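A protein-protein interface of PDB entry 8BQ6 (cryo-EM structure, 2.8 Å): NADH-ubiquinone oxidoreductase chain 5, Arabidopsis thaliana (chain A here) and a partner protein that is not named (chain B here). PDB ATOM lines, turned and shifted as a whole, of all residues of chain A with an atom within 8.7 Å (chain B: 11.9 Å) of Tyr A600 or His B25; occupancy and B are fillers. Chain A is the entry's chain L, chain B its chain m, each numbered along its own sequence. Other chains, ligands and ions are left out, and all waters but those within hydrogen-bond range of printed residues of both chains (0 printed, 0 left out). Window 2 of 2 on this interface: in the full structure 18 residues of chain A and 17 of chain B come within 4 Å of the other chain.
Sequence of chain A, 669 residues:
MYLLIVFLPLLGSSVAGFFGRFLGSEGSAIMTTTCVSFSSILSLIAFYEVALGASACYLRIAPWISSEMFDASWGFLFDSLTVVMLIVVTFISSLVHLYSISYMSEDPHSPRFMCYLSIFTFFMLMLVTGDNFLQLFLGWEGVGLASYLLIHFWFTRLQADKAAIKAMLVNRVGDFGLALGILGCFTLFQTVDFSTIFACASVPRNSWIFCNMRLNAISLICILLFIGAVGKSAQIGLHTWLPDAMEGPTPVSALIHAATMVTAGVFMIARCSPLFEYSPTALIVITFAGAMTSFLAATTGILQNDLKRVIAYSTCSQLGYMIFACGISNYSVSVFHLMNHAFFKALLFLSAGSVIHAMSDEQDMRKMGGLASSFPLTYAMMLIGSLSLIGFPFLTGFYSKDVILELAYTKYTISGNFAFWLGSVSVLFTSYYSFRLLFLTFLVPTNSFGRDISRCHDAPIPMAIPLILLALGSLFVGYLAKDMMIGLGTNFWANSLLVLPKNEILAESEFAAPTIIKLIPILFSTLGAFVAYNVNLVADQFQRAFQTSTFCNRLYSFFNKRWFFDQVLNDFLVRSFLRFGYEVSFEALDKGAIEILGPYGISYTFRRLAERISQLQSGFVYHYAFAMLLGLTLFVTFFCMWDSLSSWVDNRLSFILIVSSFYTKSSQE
The backbone carbonyl oxygen (O) of Arg B20 lies within hydrogen-bond range of the side-chain amino group (NZ) of Lys A591 (3.4 Å).
The backbone carbonyl oxygen (O) of Glu A587 is in hydrogen-bond range of the backbone NH (N) of Gly A592 (3.1 Å). O of Glu A595 sits at hydrogen-bond distance from N of Tyr A600 (3.1 Å). The backbone carbonyl oxygen (O) of Glu A595 sits at hydrogen-bond distance from the backbone NH (N) of Gly A601 (3.3 Å). The backbone carbonyl oxygen of Ile A596 lies close to the backbone NH of Gly A601 (3.4 Å). The backbone carbonyl oxygen (O) of Tyr A600 sits at hydrogen-bond distance from the side-chain hydroxyl (OG) of Ser A603 (2.9 Å). The backbone carbonyl oxygen of His B25 sits at hydrogen-bond distance from the guanidinium group of Arg B28 (2.7 Å).
Among the printed residues, merely in contact across the chains: Lys A591 with Glu B24, Lys A591 with Glu B21, Tyr A600 with His B25, Gly A592 with Phe B27, Glu A595 with Glu B24, Ile A596 with Trp B29, Lys A591 with Leu B23 and Glu A587 with Leu B23.
Gly A592 touches just one residue of chain B: Phe B27. Glu A595 touches one residue of chain B. Ile A596 touches one residue of chain B. No residue of chain B comes within 4 Å of Gly A598. No residue of chain B comes within 4 Å of Pro A599. Of the printed residues of chain B, Tyr A600 touches His B25. No residue of chain B comes within 4 Å of Gly A601. Ser A603 touches none of the printed residues of chain B. Phe A606 touches none of the printed residues of chain B. Of the printed residues of chain A, Arg B20 touches Lys A591 (3.4 Å). His B25 touches just one residue of chain A: Tyr A600 (3.4 Å). Printed residues of chain A within 4 Å of Phe B27: Gly A592 (3.4 Å). The nearest residue of chain A that does not touch His B25 is Lys A591 (5.6 Å).
Hydrophobic or aromatic side chains of chain B that line the printed part of chain A: Leu B23, His B25, Phe B27 and Trp B29. Printed residues of chain A that touch a printed residue of chain B: Glu A587, Lys A591, Gly A592, Glu A595, Ile A596 and Tyr A600. Hydrophobic or aromatic side chains of chain A that line the printed part of chain B: Ile A596 and Tyr A600. Among the printed residues, no Asp or Glu carboxylate lies within 4 Å of a Lys or Arg side-chain nitrogen of the other chain.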
ATOM      1  N   GLU A 587     -15.215   7.911  -0.425  1.00  0.00           N
ATOM      2  CA  GLU A 587     -13.828   8.359  -0.389  1.00  0.00           C
ATOM      3  C   GLU A 587     -13.023   7.837  -1.573  1.00  0.00           C
ATOM      4  O   GLU A 587     -12.267   8.588  -2.197  1.00  0.00           O
ATOM      5  CB  GLU A 587     -13.178   7.933   0.922  1.00  0.00           C
ATOM      6  CG  GLU A 587     -11.780   8.456   1.080  1.00  0.00           C
ATOM      7  CD  GLU A 587     -11.209   8.151   2.436  1.00  0.00           C
ATOM      8  OE1 GLU A 587     -11.287   6.982   2.866  1.00  0.00           O
ATOM      9  OE2 GLU A 587     -10.681   9.084   3.071  1.00  0.00           O
ATOM     10  N   ASP A 590     -16.310   8.484  -5.203  1.00  0.00           N
ATOM     11  CA  ASP A 590     -16.869   9.852  -5.424  1.00  0.00           C
ATOM     12  C   ASP A 590     -15.797  10.918  -5.180  1.00  0.00           C
ATOM     13  O   ASP A 590     -15.596  11.758  -6.069  1.00  0.00           O
ATOM     14  CB  ASP A 590     -18.121  10.117  -4.587  1.00  0.00           C
ATOM     15  CG  ASP A 590     -19.394   9.548  -5.190  1.00  0.00           C
ATOM     16  OD1 ASP A 590     -19.292   8.646  -6.045  1.00  0.00           O
ATOM     17  OD2 ASP A 590     -20.478  10.003  -4.791  1.00  0.00           O
ATOM     18  N   LYS A 591     -15.164  10.891  -4.010  1.00  0.00           N
ATOM     19  CA  LYS A 591     -14.152  11.895  -3.720  1.00  0.00           C
ATOM     20  C   LYS A 591     -12.745  11.383  -3.974  1.00  0.00           C
ATOM     21  O   LYS A 591     -11.780  11.973  -3.480  1.00  0.00           O
ATOM     22  CB  LYS A 591     -14.287  12.381  -2.277  1.00  0.00           C
ATOM     23  CG  LYS A 591     -15.541  13.202  -2.067  1.00  0.00           C
ATOM     24  CD  LYS A 591     -15.377  14.639  -2.534  1.00  0.00           C
ATOM     25  CE  LYS A 591     -15.381  15.577  -1.352  1.00  0.00           C
ATOM     26  NZ  LYS A 591     -16.501  15.213  -0.444  1.00  0.00           N
ATOM     27  N   GLY A 592     -12.615  10.289  -4.714  1.00  0.00           N
ATOM     28  CA  GLY A 592     -11.322   9.757  -5.074  1.00  0.00           C
ATOM     29  C   GLY A 592     -11.085   9.779  -6.568  1.00  0.00           C
ATOM     30  O   GLY A 592     -10.804  10.831  -7.152  1.00  0.00           O
ATOM     31  N   ALA A 593     -11.214   8.607  -7.190  1.00  0.00           N
ATOM     32  CA  ALA A 593     -10.879   8.449  -8.602  1.00  0.00           C
ATOM     33  C   ALA A 593     -11.750   9.318  -9.500  1.00  0.00           C
ATOM     34  O   ALA A 593     -11.263   9.878 -10.489  1.00  0.00           O
ATOM     35  CB  ALA A 593     -11.007   6.982  -9.002  1.00  0.00           C
ATOM     36  N   ILE A 594     -13.048   9.413  -9.201  1.00  0.00           N
ATOM     37  CA  ILE A 594     -13.934  10.228 -10.029  1.00  0.00           C
ATOM     38  C   ILE A 594     -13.521  11.692  -9.973  1.00  0.00           C
ATOM     39  O   ILE A 594     -13.581  12.406 -10.979  1.00  0.00           O
ATOM     40  CB  ILE A 594     -15.400  10.040  -9.605  1.00  0.00           C
ATOM     41  CG1 ILE A 594     -15.819   8.579  -9.746  1.00  0.00           C
ATOM     42  CG2 ILE A 594     -16.315  10.942 -10.412  1.00  0.00           C
ATOM     43  CD1 ILE A 594     -17.223   8.331  -9.286  1.00  0.00           C
ATOM     44  N   GLU A 595     -13.111  12.165  -8.796  1.00  0.00           N
ATOM     45  CA  GLU A 595     -12.608  13.529  -8.692  1.00  0.00           C
ATOM     46  C   GLU A 595     -11.290  13.695  -9.438  1.00  0.00           C
ATOM     47  O   GLU A 595     -11.108  14.670 -10.175  1.00  0.00           O
ATOM     48  CB  GLU A 595     -12.433  13.920  -7.226  1.00  0.00           C
ATOM     49  CG  GLU A 595     -13.640  14.585  -6.599  1.00  0.00           C
ATOM     50  CD  GLU A 595     -13.963  15.939  -7.204  1.00  0.00           C
ATOM     51  OE1 GLU A 595     -13.142  16.482  -7.971  1.00  0.00           O
ATOM     52  OE2 GLU A 595     -15.053  16.468  -6.909  1.00  0.00           O
ATOM     53  N   ILE A 596     -10.353  12.765  -9.243  1.00  0.00           N
ATOM     54  CA  ILE A 596      -9.056  12.877  -9.904  1.00  0.00           C
ATOM     55  C   ILE A 596      -9.213  12.751 -11.414  1.00  0.00           C
ATOM     56  O   ILE A 596      -8.641  13.539 -12.176  1.00  0.00           O
ATOM     57  CB  ILE A 596      -8.067  11.843  -9.332  1.00  0.00           C
ATOM     58  CG1 ILE A 596      -7.193  12.478  -8.248  1.00  0.00           C
ATOM     59  CG2 ILE A 596      -7.175  11.276 -10.419  1.00  0.00           C
ATOM     60  CD1 ILE A 596      -7.949  13.251  -7.202  1.00  0.00           C
ATOM     61  N   LEU A 597     -10.001  11.784 -11.873  1.00  0.00           N
ATOM     62  CA  LEU A 597     -10.294  11.676 -13.301  1.00  0.00           C
ATOM     63  C   LEU A 597     -11.548  12.466 -13.656  1.00  0.00           C
ATOM     64  O   LEU A 597     -12.452  11.988 -14.339  1.00  0.00           O
ATOM     65  CB  LEU A 597     -10.437  10.214 -13.701  1.00  0.00           C
ATOM     66  CG  LEU A 597      -9.269   9.279 -13.385  1.00  0.00           C
ATOM     67  CD1 LEU A 597      -9.464   7.956 -14.096  1.00  0.00           C
ATOM     68  CD2 LEU A 597      -7.940   9.903 -13.773  1.00  0.00           C
ATOM     69  N   GLY A 598     -11.580  13.710 -13.201  1.00  0.00           N
ATOM     70  CA  GLY A 598     -12.716  14.573 -13.387  1.00  0.00           C
ATOM     71  C   GLY A 598     -12.363  15.989 -12.995  1.00  0.00           C
ATOM     72  O   GLY A 598     -11.261  16.471 -13.268  1.00  0.00           O
ATOM     73  N   PRO A 599     -13.277  16.666 -12.296  1.00  0.00           N
ATOM     74  CA  PRO A 599     -13.101  18.113 -12.069  1.00  0.00           C
ATOM     75  C   PRO A 599     -11.804  18.487 -11.373  1.00  0.00           C
ATOM     76  O   PRO A 599     -11.193  19.503 -11.726  1.00  0.00           O
ATOM     77  CB  PRO A 599     -14.318  18.496 -11.212  1.00  0.00           C
ATOM     78  CG  PRO A 599     -15.106  17.258 -10.993  1.00  0.00           C
ATOM     79  CD  PRO A 599     -14.342  16.077 -11.472  1.00  0.00           C
ATOM     80  N   TYR A 600     -11.366  17.704 -10.386  1.00  0.00           N
ATOM     81  CA  TYR A 600     -10.168  18.075  -9.641  1.00  0.00           C
ATOM     82  C   TYR A 600      -8.915  17.924 -10.491  1.00  0.00           C
ATOM     83  O   TYR A 600      -8.072  18.827 -10.541  1.00  0.00           O
ATOM     84  CB  TYR A 600     -10.059  17.233  -8.374  1.00  0.00           C
ATOM     85  CG  TYR A 600      -8.891  17.621  -7.513  1.00  0.00           C
ATOM     86  CD1 TYR A 600      -8.846  18.856  -6.884  1.00  0.00           C
ATOM     87  CD2 TYR A 600      -7.823  16.757  -7.340  1.00  0.00           C
ATOM     88  CE1 TYR A 600      -7.772  19.213  -6.098  1.00  0.00           C
ATOM     89  CE2 TYR A 600      -6.749  17.103  -6.556  1.00  0.00           C
ATOM     90  CZ  TYR A 600      -6.726  18.331  -5.939  1.00  0.00           C
ATOM     91  OH  TYR A 600      -5.649  18.676  -5.159  1.00  0.00           O
ATOM     92  N   GLY A 601      -8.767  16.779 -11.157  1.00  0.00           N
ATOM     93  CA  GLY A 601      -7.621  16.584 -12.028  1.00  0.00           C
ATOM     94  C   GLY A 601      -7.667  17.450 -13.272  1.00  0.00           C
ATOM     95  O   GLY A 601      -6.631  17.918 -13.749  1.00  0.00           O
ATOM     96  N   ILE A 602      -8.865  17.658 -13.827  1.00  0.00           N
ATOM     97  CA  ILE A 602      -8.998  18.421 -15.067  1.00  0.00           C
ATOM     98  C   ILE A 602      -8.623  19.880 -14.844  1.00  0.00           C
ATOM     99  O   ILE A 602      -7.980  20.509 -15.694  1.00  0.00           O
ATOM    100  CB  ILE A 602     -10.424  18.276 -15.632  1.00  0.00           C
ATOM    101  CG1 ILE A 602     -10.555  16.966 -16.412  1.00  0.00           C
ATOM    102  CG2 ILE A 602     -10.799  19.461 -16.501  1.00  0.00           C
ATOM    103  CD1 ILE A 602     -11.952  16.421 -16.444  1.00  0.00           C
ATOM    104  N   SER A 603      -9.028  20.445 -13.706  1.00  0.00           N
ATOM    105  CA  SER A 603      -8.631  21.810 -13.383  1.00  0.00           C
ATOM    106  C   SER A 603      -7.122  21.919 -13.212  1.00  0.00           C
ATOM    107  O   SER A 603      -6.505  22.886 -13.669  1.00  0.00           O
ATOM    108  CB  SER A 603      -9.347  22.279 -12.119  1.00  0.00           C
ATOM    109  OG  SER A 603      -8.953  21.513 -10.997  1.00  0.00           O
ATOM    110  N   TYR A 604      -6.511  20.929 -12.559  1.00  0.00           N
ATOM    111  CA  TYR A 604      -5.071  20.961 -12.321  1.00  0.00           C
ATOM    112  C   TYR A 604      -4.291  20.971 -13.636  1.00  0.00           C
ATOM    113  O   TYR A 604      -3.438  21.844 -13.868  1.00  0.00           O
ATOM    114  CB  TYR A 604      -4.673  19.748 -11.483  1.00  0.00           C
ATOM    115  CG  TYR A 604      -3.220  19.723 -11.102  1.00  0.00           C
ATOM    116  CD1 TYR A 604      -2.665  20.736 -10.338  1.00  0.00           C
ATOM    117  CD2 TYR A 604      -2.385  18.719 -11.570  1.00  0.00           C
ATOM    118  CE1 TYR A 604      -1.335  20.716  -9.996  1.00  0.00           C
ATOM    119  CE2 TYR A 604      -1.048  18.698 -11.247  1.00  0.00           C
ATOM    120  CZ  TYR A 604      -0.526  19.702 -10.463  1.00  0.00           C
ATOM    121  OH  TYR A 604       0.808  19.683 -10.137  1.00  0.00           O
ATOM    122  N   THR A 605      -4.581  20.007 -14.514  1.00  0.00           N
ATOM    123  CA  THR A 605      -3.830  19.898 -15.760  1.00  0.00           C
ATOM    124  C   THR A 605      -4.050  21.115 -16.646  1.00  0.00           C
ATOM    125  O   THR A 605      -3.113  21.590 -17.298  1.00  0.00           O
ATOM    126  CB  THR A 605      -4.199  18.618 -16.513  1.00  0.00           C
ATOM    127  OG1 THR A 605      -3.636  18.664 -17.829  1.00  0.00           O
ATOM    128  CG2 THR A 605      -5.698  18.468 -16.645  1.00  0.00           C
ATOM    129  N   PHE A 606      -5.274  21.638 -16.688  1.00  0.00           N
ATOM    130  CA  PHE A 606      -5.516  22.780 -17.558  1.00  0.00           C
ATOM    131  C   PHE A 606      -4.928  24.056 -16.979  1.00  0.00           C
ATOM    132  O   PHE A 606      -4.521  24.940 -17.735  1.00  0.00           O
ATOM    133  CB  PHE A 606      -7.006  22.918 -17.845  1.00  0.00           C
ATOM    134  CG  PHE A 606      -7.435  22.151 -19.055  1.00  0.00           C
ATOM    135  CD1 PHE A 606      -7.145  22.618 -20.322  1.00  0.00           C
ATOM    136  CD2 PHE A 606      -8.063  20.927 -18.925  1.00  0.00           C
ATOM    137  CE1 PHE A 606      -7.517  21.898 -21.440  1.00  0.00           C
ATOM    138  CE2 PHE A 606      -8.435  20.202 -20.037  1.00  0.00           C
ATOM    139  CZ  PHE A 606      -8.161  20.686 -21.295  1.00  0.00           C
ATOM    140  N   ARG A 607      -4.829  24.153 -15.653  1.00  0.00           N
ATOM    141  CA  ARG A 607      -4.120  25.279 -15.055  1.00  0.00           C
ATOM    142  C   ARG A 607      -2.640  25.248 -15.425  1.00  0.00           C
ATOM    143  O   ARG A 607      -2.056  26.282 -15.766  1.00  0.00           O
ATOM    144  CB  ARG A 607      -4.311  25.270 -13.539  1.00  0.00           C
ATOM    145  CG  ARG A 607      -5.609  25.919 -13.088  1.00  0.00           C
ATOM    146  CD  ARG A 607      -5.572  26.323 -11.629  1.00  0.00           C
ATOM    147  NE  ARG A 607      -5.986  25.236 -10.749  1.00  0.00           N
ATOM    148  CZ  ARG A 607      -5.187  24.642  -9.875  1.00  0.00           C
ATOM    149  NH1 ARG A 607      -3.924  25.006  -9.738  1.00  0.00           N
ATOM    150  NH2 ARG A 607      -5.668  23.663  -9.116  1.00  0.00           N
ATOM    151  N   ASP B  15     -14.185  21.612  12.222  1.00  0.00           N
ATOM    152  CA  ASP B  15     -13.014  21.023  11.576  1.00  0.00           C
ATOM    153  C   ASP B  15     -13.340  19.659  10.995  1.00  0.00           C
ATOM    154  O   ASP B  15     -12.927  19.329   9.876  1.00  0.00           O
ATOM    155  CB  ASP B  15     -11.875  20.897  12.581  1.00  0.00           C
ATOM    156  CG  ASP B  15     -11.041  22.143  12.664  1.00  0.00           C
ATOM    157  OD1 ASP B  15     -11.521  23.201  12.214  1.00  0.00           O
ATOM    158  OD2 ASP B  15      -9.910  22.067  13.183  1.00  0.00           O
ATOM    159  N   GLY B  17     -16.245  18.868   9.996  1.00  0.00           N
ATOM    160  CA  GLY B  17     -17.087  19.145   8.843  1.00  0.00           C
ATOM    161  C   GLY B  17     -16.294  19.541   7.611  1.00  0.00           C
ATOM    162  O   GLY B  17     -16.584  19.092   6.500  1.00  0.00           O
ATOM    163  N   SER B  18     -15.283  20.395   7.789  1.00  0.00           N
ATOM    164  CA  SER B  18     -14.502  20.849   6.643  1.00  0.00           C
ATOM    165  C   SER B  18     -13.597  19.752   6.098  1.00  0.00           C
ATOM    166  O   SER B  18     -13.347  19.704   4.888  1.00  0.00           O
ATOM    167  CB  SER B  18     -13.670  22.073   7.017  1.00  0.00           C
ATOM    168  OG  SER B  18     -13.012  21.881   8.254  1.00  0.00           O
ATOM    169  N   ALA B  19     -13.083  18.878   6.964  1.00  0.00           N
ATOM    170  CA  ALA B  19     -12.228  17.798   6.486  1.00  0.00           C
ATOM    171  C   ALA B  19     -13.021  16.806   5.644  1.00  0.00           C
ATOM    172  O   ALA B  19     -12.464  16.144   4.761  1.00  0.00           O
ATOM    173  CB  ALA B  19     -11.557  17.094   7.664  1.00  0.00           C
ATOM    174  N   ARG B  20     -14.323  16.682   5.912  1.00  0.00           N
ATOM    175  CA  ARG B  20     -15.168  15.830   5.084  1.00  0.00           C
ATOM    176  C   ARG B  20     -15.364  16.411   3.693  1.00  0.00           C
ATOM    177  O   ARG B  20     -15.300  15.685   2.693  1.00  0.00           O
ATOM    178  CB  ARG B  20     -16.522  15.626   5.749  1.00  0.00           C
ATOM    179  CG  ARG B  20     -17.406  14.719   4.959  1.00  0.00           C
ATOM    180  CD  ARG B  20     -16.725  13.399   4.750  1.00  0.00           C
ATOM    181  NE  ARG B  20     -16.370  12.803   6.027  1.00  0.00           N
ATOM    182  CZ  ARG B  20     -17.190  12.070   6.762  1.00  0.00           C
ATOM    183  NH1 ARG B  20     -18.423  11.807   6.366  1.00  0.00           N
ATOM    184  NH2 ARG B  20     -16.758  11.583   7.918  1.00  0.00           N
ATOM    185  N   GLU B  21     -15.633  17.713   3.609  1.00  0.00           N
ATOM    186  CA  GLU B  21     -15.868  18.364   2.327  1.00  0.00           C
ATOM    187  C   GLU B  21     -14.641  18.359   1.425  1.00  0.00           C
ATOM    188  O   GLU B  21     -14.794  18.424   0.201  1.00  0.00           O
ATOM    189  CB  GLU B  21     -16.332  19.806   2.552  1.00  0.00           C
ATOM    190  CG  GLU B  21     -17.842  19.975   2.634  1.00  0.00           C
ATOM    191  CD  GLU B  21     -18.262  21.138   3.517  1.00  0.00           C
ATOM    192  OE1 GLU B  21     -19.429  21.571   3.409  1.00  0.00           O
ATOM    193  OE2 GLU B  21     -17.433  21.618   4.319  1.00  0.00           O
ATOM    194  N   ASN B  22     -13.441  18.278   1.993  1.00  0.00           N
ATOM    195  CA  ASN B  22     -12.190  18.441   1.262  1.00  0.00           C
ATOM    196  C   ASN B  22     -11.446  17.120   1.162  1.00  0.00           C
ATOM    197  O   ASN B  22     -10.227  17.054   1.344  1.00  0.00           O
ATOM    198  CB  ASN B  22     -11.310  19.498   1.920  1.00  0.00           C
ATOM    199  CG  ASN B  22     -11.921  20.879   1.859  1.00  0.00           C
ATOM    200  OD1 ASN B  22     -12.215  21.481   2.890  1.00  0.00           O
ATOM    201  ND2 ASN B  22     -12.108  21.393   0.651  1.00  0.00           N
ATOM    202  N   LEU B  23     -12.173  16.040   0.898  1.00  0.00           N
ATOM    203  CA  LEU B  23     -11.542  14.727   0.893  1.00  0.00           C
ATOM    204  C   LEU B  23     -10.710  14.502  -0.364  1.00  0.00           C
ATOM    205  O   LEU B  23      -9.743  13.732  -0.332  1.00  0.00           O
ATOM    206  CB  LEU B  23     -12.610  13.649   1.029  1.00  0.00           C
ATOM    207  CG  LEU B  23     -12.293  12.492   1.968  1.00  0.00           C
ATOM    208  CD1 LEU B  23     -11.525  13.002   3.172  1.00  0.00           C
ATOM    209  CD2 LEU B  23     -13.580  11.814   2.394  1.00  0.00           C
ATOM    210  N   GLU B  24     -11.061  15.162  -1.470  1.00  0.00           N
ATOM    211  CA  GLU B  24     -10.374  14.918  -2.733  1.00  0.00           C
ATOM    212  C   GLU B  24      -8.919  15.366  -2.700  1.00  0.00           C
ATOM    213  O   GLU B  24      -8.119  14.893  -3.515  1.00  0.00           O
ATOM    214  CB  GLU B  24     -11.105  15.617  -3.882  1.00  0.00           C
ATOM    215  CG  GLU B  24     -11.304  17.111  -3.694  1.00  0.00           C
ATOM    216  CD  GLU B  24     -12.631  17.443  -3.050  1.00  0.00           C
ATOM    217  OE1 GLU B  24     -13.579  17.798  -3.780  1.00  0.00           O
ATOM    218  OE2 GLU B  24     -12.725  17.346  -1.810  1.00  0.00           O
ATOM    219  N   HIS B  25      -8.556  16.261  -1.784  1.00  0.00           N
ATOM    220  CA  HIS B  25      -7.154  16.627  -1.632  1.00  0.00           C
ATOM    221  C   HIS B  25      -6.333  15.530  -0.972  1.00  0.00           C
ATOM    222  O   HIS B  25      -5.101  15.623  -0.970  1.00  0.00           O
ATOM    223  CB  HIS B  25      -7.028  17.919  -0.825  1.00  0.00           C
ATOM    224  CG  HIS B  25      -7.783  19.071  -1.408  1.00  0.00           C
ATOM    225  ND1 HIS B  25      -8.735  19.772  -0.701  1.00  0.00           N
ATOM    226  CD2 HIS B  25      -7.729  19.642  -2.634  1.00  0.00           C
ATOM    227  CE1 HIS B  25      -9.235  20.725  -1.466  1.00  0.00           C
ATOM    228  NE2 HIS B  25      -8.642  20.667  -2.645  1.00  0.00           N
ATOM    229  N   ASN B  26      -6.974  14.499  -0.422  1.00  0.00           N
ATOM    230  CA  ASN B  26      -6.273  13.452   0.309  1.00  0.00           C
ATOM    231  C   ASN B  26      -6.000  12.204  -0.518  1.00  0.00           C
ATOM    232  O   ASN B  26      -5.200  11.368  -0.089  1.00  0.00           O
ATOM    233  CB  ASN B  26      -7.068  13.051   1.556  1.00  0.00           C
ATOM    234  CG  ASN B  26      -7.188  14.177   2.555  1.00  0.00           C
ATOM    235  OD1 ASN B  26      -6.891  15.331   2.249  1.00  0.00           O
ATOM    236  ND2 ASN B  26      -7.623  13.846   3.764  1.00  0.00           N
ATOM    237  N   PHE B  27      -6.648  12.047  -1.670  1.00  0.00           N
ATOM    238  CA  PHE B  27      -6.459  10.850  -2.479  1.00  0.00           C
ATOM    239  C   PHE B  27      -4.997  10.706  -2.888  1.00  0.00           C
ATOM    240  O   PHE B  27      -4.373  11.667  -3.345  1.00  0.00           O
ATOM    241  CB  PHE B  27      -7.354  10.915  -3.713  1.00  0.00           C
ATOM    242  CG  PHE B  27      -7.484   9.611  -4.428  1.00  0.00           C
ATOM    243  CD1 PHE B  27      -8.294   8.611  -3.926  1.00  0.00           C
ATOM    244  CD2 PHE B  27      -6.778   9.378  -5.591  1.00  0.00           C
ATOM    245  CE1 PHE B  27      -8.411   7.411  -4.579  1.00  0.00           C
ATOM    246  CE2 PHE B  27      -6.888   8.178  -6.247  1.00  0.00           C
ATOM    247  CZ  PHE B  27      -7.705   7.192  -5.741  1.00  0.00           C
ATOM    248  N   ARG B  28      -4.447   9.497  -2.727  1.00  0.00           N
ATOM    249  CA  ARG B  28      -3.014   9.297  -2.903  1.00  0.00           C
ATOM    250  C   ARG B  28      -2.631   8.219  -3.913  1.00  0.00           C
ATOM    251  O   ARG B  28      -1.459   8.165  -4.303  1.00  0.00           O
ATOM    252  CB  ARG B  28      -2.355   8.971  -1.551  1.00  0.00           C
ATOM    253  CG  ARG B  28      -2.195  10.172  -0.626  1.00  0.00           C
ATOM    254  CD  ARG B  28      -1.206  11.196  -1.173  1.00  0.00           C
ATOM    255  NE  ARG B  28      -1.864  12.277  -1.900  1.00  0.00           N
ATOM    256  CZ  ARG B  28      -2.522  13.278  -1.331  1.00  0.00           C
ATOM    257  NH1 ARG B  28      -2.629  13.376  -0.016  1.00  0.00           N
ATOM    258  NH2 ARG B  28      -3.090  14.201  -2.101  1.00  0.00           N
ATOM    259  N   TRP B  29      -3.578   7.389  -4.365  1.00  0.00           N
ATOM    260  CA  TRP B  29      -3.319   6.267  -5.278  1.00  0.00           C
ATOM    261  C   TRP B  29      -2.427   5.207  -4.620  1.00  0.00           C
ATOM    262  O   TRP B  29      -1.357   4.856  -5.120  1.00  0.00           O
ATOM    263  CB  TRP B  29      -2.705   6.742  -6.605  1.00  0.00           C
ATOM    264  CG  TRP B  29      -3.670   7.298  -7.626  1.00  0.00           C
ATOM    265  CD1 TRP B  29      -3.660   8.555  -8.158  1.00  0.00           C
ATOM    266  CD2 TRP B  29      -4.758   6.609  -8.254  1.00  0.00           C
ATOM    267  NE1 TRP B  29      -4.680   8.695  -9.067  1.00  0.00           N
ATOM    268  CE2 TRP B  29      -5.369   7.514  -9.144  1.00  0.00           C
ATOM    269  CE3 TRP B  29      -5.282   5.319  -8.142  1.00  0.00           C
ATOM    270  CZ2 TRP B  29      -6.476   7.171  -9.915  1.00  0.00           C
ATOM    271  CZ3 TRP B  29      -6.379   4.981  -8.910  1.00  0.00           C
ATOM    272  CH2 TRP B  29      -6.963   5.902  -9.785  1.00  0.00           C
ATOM    273  N   THR B  30      -2.900   4.686  -3.490  1.00  0.00           N
ATOM    274  CA  THR B  30      -2.169   3.674  -2.742  1.00  0.00           C
ATOM    275  C   THR B  30      -2.563   2.271  -3.207  1.00  0.00           C
ATOM    276  O   THR B  30      -3.350   2.093  -4.140  1.00  0.00           O
ATOM    277  CB  THR B  30      -2.411   3.851  -1.243  1.00  0.00           C
ATOM    278  OG1 THR B  30      -3.720   3.378  -0.909  1.00  0.00           O
ATOM    279  CG2 THR B  30      -2.309   5.315  -0.864  1.00  0.00           C
ATOM    280  N   ASN B  33      -6.325   1.666  -2.261  1.00  0.00           N
ATOM    281  CA  ASN B  33      -7.211   2.367  -3.182  1.00  0.00           C
ATOM    282  C   ASN B  33      -7.270   1.664  -4.531  1.00  0.00           C
ATOM    283  O   ASN B  33      -8.344   1.543  -5.129  1.00  0.00           O
ATOM    284  CB  ASN B  33      -6.748   3.811  -3.350  1.00  0.00           C
ATOM    285  CG  ASN B  33      -7.349   4.734  -2.319  1.00  0.00           C
ATOM    286  OD1 ASN B  33      -8.335   4.395  -1.665  1.00  0.00           O
ATOM    287  ND2 ASN B  33      -6.757   5.909  -2.164  1.00  0.00           N
